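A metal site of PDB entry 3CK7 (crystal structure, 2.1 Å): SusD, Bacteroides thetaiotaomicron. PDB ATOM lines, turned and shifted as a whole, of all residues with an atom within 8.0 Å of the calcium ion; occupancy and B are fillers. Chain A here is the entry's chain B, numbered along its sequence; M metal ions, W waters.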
ATOM      1  N   PHE A 191     -14.794  -0.620  -7.407  1.00  0.00           N
ATOM      2  CA  PHE A 191     -15.290   0.398  -6.480  1.00  0.00           C
ATOM      3  C   PHE A 191     -14.270   1.503  -6.280  1.00  0.00           C
ATOM      4  O   PHE A 191     -13.137   1.253  -5.864  1.00  0.00           O
ATOM      5  CB  PHE A 191     -15.661  -0.222  -5.129  1.00  0.00           C
ATOM      6  CG  PHE A 191     -16.482   0.700  -4.256  1.00  0.00           C
ATOM      7  CD1 PHE A 191     -17.746   1.103  -4.662  1.00  0.00           C
ATOM      8  CD2 PHE A 191     -15.974   1.186  -3.056  1.00  0.00           C
ATOM      9  CE1 PHE A 191     -18.505   1.985  -3.880  1.00  0.00           C
ATOM     10  CE2 PHE A 191     -16.717   2.068  -2.261  1.00  0.00           C
ATOM     11  CZ  PHE A 191     -17.984   2.464  -2.679  1.00  0.00           C
ATOM     12  N   MET A 245     -21.659   5.712   7.010  1.00  0.00           N
ATOM     13  CA  MET A 245     -20.996   4.931   8.050  1.00  0.00           C
ATOM     14  C   MET A 245     -19.650   4.341   7.590  1.00  0.00           C
ATOM     15  O   MET A 245     -19.332   4.354   6.407  1.00  0.00           O
ATOM     16  CB  MET A 245     -21.929   3.828   8.568  1.00  0.00           C
ATOM     17  CG  MET A 245     -23.046   4.378   9.446  1.00  0.00           C
ATOM     18  SD  MET A 245     -24.308   3.167   9.851  1.00  0.00           S
ATOM     19  CE  MET A 245     -23.564   2.339  11.207  1.00  0.00           C
ATOM     20  N   ALA A 246     -18.874   3.835   8.539  1.00  0.00           N
ATOM     21  CA  ALA A 246     -17.542   3.300   8.284  1.00  0.00           C
ATOM     22  C   ALA A 246     -17.404   2.149   7.282  1.00  0.00           C
ATOM     23  O   ALA A 246     -16.329   1.937   6.734  1.00  0.00           O
ATOM     24  CB  ALA A 246     -16.887   2.920   9.595  1.00  0.00           C
ATOM     25  N   ASP A 247     -18.484   1.410   7.053  1.00  0.00           N
ATOM     26  CA  ASP A 247     -18.420   0.293   6.123  1.00  0.00           C
ATOM     27  C   ASP A 247     -19.188   0.585   4.829  1.00  0.00           C
ATOM     28  O   ASP A 247     -19.653  -0.336   4.157  1.00  0.00           O
ATOM     29  CB  ASP A 247     -18.945  -0.975   6.799  1.00  0.00           C
ATOM     30  CG  ASP A 247     -20.378  -0.846   7.268  1.00  0.00           C
ATOM     31  OD1 ASP A 247     -20.804   0.269   7.659  1.00  0.00           O
ATOM     32  OD2 ASP A 247     -21.093  -1.869   7.259  1.00  0.00           O
ATOM     33  N   ASN A 248     -19.309   1.859   4.471  1.00  0.00           N
ATOM     34  CA  ASN A 248     -20.019   2.231   3.260  1.00  0.00           C
ATOM     35  C   ASN A 248     -19.301   1.827   1.974  1.00  0.00           C
ATOM     36  O   ASN A 248     -19.734   2.166   0.884  1.00  0.00           O
ATOM     37  CB  ASN A 248     -20.342   3.739   3.246  1.00  0.00           C
ATOM     38  CG  ASN A 248     -19.096   4.617   3.341  1.00  0.00           C
ATOM     39  OD1 ASN A 248     -17.992   4.143   3.600  1.00  0.00           O
ATOM     40  ND2 ASN A 248     -19.291   5.915   3.153  1.00  0.00           N
ATOM     41  N   ASP A 249     -18.198   1.094   2.124  1.00  0.00           N
ATOM     42  CA  ASP A 249     -17.450   0.616   0.965  1.00  0.00           C
ATOM     43  C   ASP A 249     -17.533  -0.914   0.876  1.00  0.00           C
ATOM     44  O   ASP A 249     -17.027  -1.518  -0.073  1.00  0.00           O
ATOM     45  CB  ASP A 249     -15.981   1.088   1.033  1.00  0.00           C
ATOM     46  CG  ASP A 249     -15.223   0.501   2.215  1.00  0.00           C
ATOM     47  OD1 ASP A 249     -15.852  -0.074   3.134  1.00  0.00           O
ATOM     48  OD2 ASP A 249     -13.984   0.636   2.237  1.00  0.00           O
ATOM     49  N   GLU A 250     -18.201  -1.516   1.861  1.00  0.00           N
ATOM     50  CA  GLU A 250     -18.378  -2.967   1.914  1.00  0.00           C
ATOM     51  C   GLU A 250     -19.860  -3.318   2.012  1.00  0.00           C
ATOM     52  O   GLU A 250     -20.283  -4.378   1.551  1.00  0.00           O
ATOM     53  CB  GLU A 250     -17.643  -3.549   3.124  1.00  0.00           C
ATOM     54  CG  GLU A 250     -16.139  -3.564   2.989  1.00  0.00           C
ATOM     55  CD  GLU A 250     -15.444  -3.961   4.285  1.00  0.00           C
ATOM     56  OE1 GLU A 250     -15.862  -4.976   4.892  1.00  0.00           O
ATOM     57  OE2 GLU A 250     -14.488  -3.267   4.683  1.00  0.00           O
ATOM     58  N   ILE A 262     -15.067   8.718  -2.401  1.00  0.00           N
ATOM     59  CA  ILE A 262     -13.706   9.224  -2.170  1.00  0.00           C
ATOM     60  C   ILE A 262     -13.248   8.282  -1.058  1.00  0.00           C
ATOM     61  O   ILE A 262     -13.689   8.401   0.095  1.00  0.00           O
ATOM     62  CB  ILE A 262     -13.672  10.676  -1.636  1.00  0.00           C
ATOM     63  CG1 ILE A 262     -14.173  11.648  -2.698  1.00  0.00           C
ATOM     64  CG2 ILE A 262     -12.227  11.042  -1.278  1.00  0.00           C
ATOM     65  CD1 ILE A 262     -14.117  13.120  -2.255  1.00  0.00           C
ATOM     66  N   ARG A 263     -12.405   7.320  -1.415  1.00  0.00           N
ATOM     67  CA  ARG A 263     -11.916   6.330  -0.465  1.00  0.00           C
ATOM     68  C   ARG A 263     -11.190   6.911   0.748  1.00  0.00           C
ATOM     69  O   ARG A 263     -10.389   7.840   0.625  1.00  0.00           O
ATOM     70  CB  ARG A 263     -11.000   5.324  -1.179  1.00  0.00           C
ATOM     71  CG  ARG A 263     -11.609   4.704  -2.438  1.00  0.00           C
ATOM     72  CD  ARG A 263     -13.021   4.183  -2.192  1.00  0.00           C
ATOM     73  NE  ARG A 263     -13.058   3.168  -1.150  1.00  0.00           N
ATOM     74  CZ  ARG A 263     -12.618   1.924  -1.296  1.00  0.00           C
ATOM     75  NH1 ARG A 263     -12.105   1.527  -2.456  1.00  0.00           N
ATOM     76  NH2 ARG A 263     -12.682   1.078  -0.277  1.00  0.00           N
ATOM     77  N   GLN A 264     -11.459   6.341   1.922  1.00  0.00           N
ATOM     78  CA  GLN A 264     -10.852   6.790   3.162  1.00  0.00           C
ATOM     79  C   GLN A 264     -10.581   5.586   4.060  1.00  0.00           C
ATOM     80  O   GLN A 264     -11.328   4.610   4.039  1.00  0.00           O
ATOM     81  CB  GLN A 264     -11.795   7.773   3.879  1.00  0.00           C
ATOM     82  CG  GLN A 264     -12.086   9.029   3.080  1.00  0.00           C
ATOM     83  CD  GLN A 264     -10.963  10.041   3.144  1.00  0.00           C
ATOM     84  OE1 GLN A 264     -10.900  10.849   4.063  1.00  0.00           O
ATOM     85  NE2 GLN A 264     -10.051   9.988   2.170  1.00  0.00           N
ATOM     86  N   ASP A 265      -9.514   5.657   4.838  1.00  0.00           N
ATOM     87  CA  ASP A 265      -9.172   4.551   5.722  1.00  0.00           C
ATOM     88  C   ASP A 265      -8.455   5.066   6.966  1.00  0.00           C
ATOM     89  O   ASP A 265      -7.453   5.776   6.864  1.00  0.00           O
ATOM     90  CB  ASP A 265      -8.314   3.549   4.952  1.00  0.00           C
ATOM     91  CG  ASP A 265      -8.040   2.292   5.755  1.00  0.00           C
ATOM     92  OD1 ASP A 265      -7.017   2.249   6.451  1.00  0.00           O
ATOM     93  OD2 ASP A 265      -8.866   1.361   5.703  1.00  0.00           O
ATOM     94  N   GLY A 266      -8.969   4.704   8.127  1.00  0.00           N
ATOM     95  CA  GLY A 266      -8.384   5.158   9.377  1.00  0.00           C
ATOM     96  C   GLY A 266      -6.889   4.934   9.505  1.00  0.00           C
ATOM     97  O   GLY A 266      -6.177   5.758  10.084  1.00  0.00           O
ATOM     98  N   THR A 269      -5.590   5.639   4.726  1.00  0.00           N
ATOM     99  CA  THR A 269      -5.890   6.884   4.019  1.00  0.00           C
ATOM    100  C   THR A 269      -6.281   8.009   4.968  1.00  0.00           C
ATOM    101  O   THR A 269      -7.477   8.236   5.220  1.00  0.00           O
ATOM    102  CB  THR A 269      -7.026   6.674   2.987  1.00  0.00           C
ATOM    103  OG1 THR A 269      -6.742   5.521   2.185  1.00  0.00           O
ATOM    104  CG2 THR A 269      -7.155   7.898   2.070  1.00  0.00           C
ATOM    105  N   SER A 275     -12.787  12.406   5.572  1.00  0.00           N
ATOM    106  CA  SER A 275     -13.849  11.974   6.475  1.00  0.00           C
ATOM    107  C   SER A 275     -13.464  12.306   7.915  1.00  0.00           C
ATOM    108  O   SER A 275     -14.329  12.444   8.780  1.00  0.00           O
ATOM    109  CB  SER A 275     -14.131  10.466   6.328  1.00  0.00           C
ATOM    110  OG  SER A 275     -12.971   9.693   6.520  1.00  0.00           O
ATOM    111  N   ASN A 391     -18.216   7.021  12.448  1.00  0.00           N
ATOM    112  CA  ASN A 391     -17.119   6.086  12.299  1.00  0.00           C
ATOM    113  C   ASN A 391     -17.496   4.766  12.971  1.00  0.00           C
ATOM    114  O   ASN A 391     -16.773   4.239  13.811  1.00  0.00           O
ATOM    115  CB  ASN A 391     -15.807   6.574  12.909  1.00  0.00           C
ATOM    116  CG  ASN A 391     -14.636   5.690  12.523  1.00  0.00           C
ATOM    117  OD1 ASN A 391     -13.617   5.604  13.211  1.00  0.00           O
ATOM    118  ND2 ASN A 391     -14.773   5.019  11.385  1.00  0.00           N
ATOM    119  N   ARG A 393     -19.436   0.910  11.852  1.00  0.00           N
ATOM    120  CA  ARG A 393     -19.877   0.079  10.733  1.00  0.00           C
ATOM    121  C   ARG A 393     -21.307  -0.380  10.980  1.00  0.00           C
ATOM    122  O   ARG A 393     -21.695  -0.611  12.121  1.00  0.00           O
ATOM    123  CB  ARG A 393     -18.991  -1.151  10.593  1.00  0.00           C
ATOM    124  CG  ARG A 393     -17.560  -0.869  10.165  1.00  0.00           C
ATOM    125  CD  ARG A 393     -16.746  -2.147  10.226  1.00  0.00           C
ATOM    126  NE  ARG A 393     -17.260  -3.177   9.320  1.00  0.00           N
ATOM    127  CZ  ARG A 393     -16.753  -3.410   8.110  1.00  0.00           C
ATOM    128  NH1 ARG A 393     -15.730  -2.686   7.680  1.00  0.00           N
ATOM    129  NH2 ARG A 393     -17.267  -4.359   7.341  1.00  0.00           N
ATOM    130  N   SER A 400     -10.883   0.223  11.563  1.00  0.00           N
ATOM    131  CA  SER A 400      -9.436   0.104  11.617  1.00  0.00           C
ATOM    132  C   SER A 400      -8.652   0.997  12.580  1.00  0.00           C
ATOM    133  O   SER A 400      -7.539   0.654  12.962  1.00  0.00           O
ATOM    134  CB  SER A 400      -8.828   0.312  10.223  1.00  0.00           C
ATOM    135  OG  SER A 400      -8.796   1.683   9.908  1.00  0.00           O
ATOM    136  N   PRO A 405     -11.315   7.950  10.936  1.00  0.00           N
ATOM    137  CA  PRO A 405     -12.409   7.106  10.429  1.00  0.00           C
ATOM    138  C   PRO A 405     -12.126   6.333   9.146  1.00  0.00           C
ATOM    139  O   PRO A 405     -11.256   6.703   8.355  1.00  0.00           O
ATOM    140  CB  PRO A 405     -13.534   8.101  10.243  1.00  0.00           C
ATOM    141  CG  PRO A 405     -12.798   9.321   9.787  1.00  0.00           C
ATOM    142  CD  PRO A 405     -11.618   9.367  10.728  1.00  0.00           C
ATOM    143  N   ASP A 406     -12.881   5.258   8.935  1.00  0.00           N
ATOM    144  CA  ASP A 406     -12.747   4.441   7.727  1.00  0.00           C
ATOM    145  C   ASP A 406     -13.816   4.902   6.746  1.00  0.00           C
ATOM    146  O   ASP A 406     -13.794   4.544   5.568  1.00  0.00           O
ATOM    147  CB  ASP A 406     -12.991   2.954   8.024  1.00  0.00           C
ATOM    148  CG  ASP A 406     -11.896   2.337   8.873  1.00  0.00           C
ATOM    149  OD1 ASP A 406     -10.787   2.913   8.981  1.00  0.00           O
ATOM    150  OD2 ASP A 406     -12.154   1.237   9.417  1.00  0.00           O
ATOM    151  N   THR A 407     -14.750   5.702   7.241  1.00  0.00           N
ATOM    152  CA  THR A 407     -15.854   6.190   6.427  1.00  0.00           C
ATOM    153  C   THR A 407     -15.429   6.863   5.134  1.00  0.00           C
ATOM    154  O   THR A 407     -14.673   7.840   5.143  1.00  0.00           O
ATOM    155  CB  THR A 407     -16.728   7.161   7.234  1.00  0.00           C
ATOM    156  OG1 THR A 407     -17.040   6.590   8.510  1.00  0.00           O
ATOM    157  CG2 THR A 407     -18.017   7.447   6.486  1.00  0.00           C
ATOM    158  N   ASP A 408     -15.919   6.340   4.008  1.00  0.00           N
ATOM    159  CA  ASP A 408     -15.622   6.925   2.703  1.00  0.00           C
ATOM    160  C   ASP A 408     -16.578   8.110   2.536  1.00  0.00           C
ATOM    161  O   ASP A 408     -17.577   8.216   3.235  1.00  0.00           O
ATOM    162  CB  ASP A 408     -15.889   5.931   1.572  1.00  0.00           C
ATOM    163  CG  ASP A 408     -14.773   4.935   1.387  1.00  0.00           C
ATOM    164  OD1 ASP A 408     -13.707   5.120   1.985  1.00  0.00           O
ATOM    165  OD2 ASP A 408     -14.969   3.961   0.626  1.00  0.00           O
ATOM    166  N   ILE A 409     -16.247   8.996   1.600  1.00  0.00           N
ATOM    167  CA  ILE A 409     -17.102  10.152   1.310  1.00  0.00           C
ATOM    168  C   ILE A 409     -17.891   9.859   0.031  1.00  0.00           C
ATOM    169  O   ILE A 409     -17.329   9.818  -1.070  1.00  0.00           O
ATOM    170  CB  ILE A 409     -16.241  11.429   1.108  1.00  0.00           C
ATOM    171  CG1 ILE A 409     -15.639  11.860   2.451  1.00  0.00           C
ATOM    172  CG2 ILE A 409     -17.093  12.546   0.517  1.00  0.00           C
ATOM    173  CD1 ILE A 409     -14.694  13.061   2.373  1.00  0.00           C
HETATM  174 CA    CA M   1     -13.167   3.214   3.785  1.00  0.00          CA
HETATM  175  O   HOH W   1     -15.932   2.727   4.153  1.00  0.00           O
HETATM  176  O   HOH W   2     -12.136   1.418   5.245  1.00  0.00           O
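The backbone NH of Gly 266 sits at hydrogen-bond distance from the side-chain carboxylate of Asp 406.
The side-chain carboxylate (OD1) of Asp 406 is in hydrogen-bond range of the side-chain hydroxyl (OG) of Ser 400 (2.5 Å).
The backbone NH (N) of Asp 406 sits close to the side-chain amide nitrogen (ND2) of Asn 391 (3.1 Å).
The backbone NH (N) of Ser 275 is in hydrogen-bond range of the side-chain amide oxygen (OE1) of Gln 264, 2.9 Å away.
OD2 of Asp 408 lies within salt-bridge range of NE of Arg 263, at 2.7 Å.
O of Asp 408 is in hydrogen-bond range of ND2 of Asn 248 (2.9 Å).
NH2 of Arg 263 lies within salt-bridge range of OD2 of Asp 249 (2.9 Å).
Of the 22 residues printed, 4 come within 4 Å of the calcium ion.
The calcium ion is bound by the backbone carbonyl oxygen of Asp 406 (2.3 Å), the backbone carbonyl oxygen of Gln 264 (2.3 Å), water W2 (2.5 Å), the side-chain carboxylate of Asp 408 (2.7 Å) and water W1 (2.8 Å).
Slightly farther from the calcium ion lies the side-chain carboxylate (OD2) of Asp 249 (3.1 Å).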
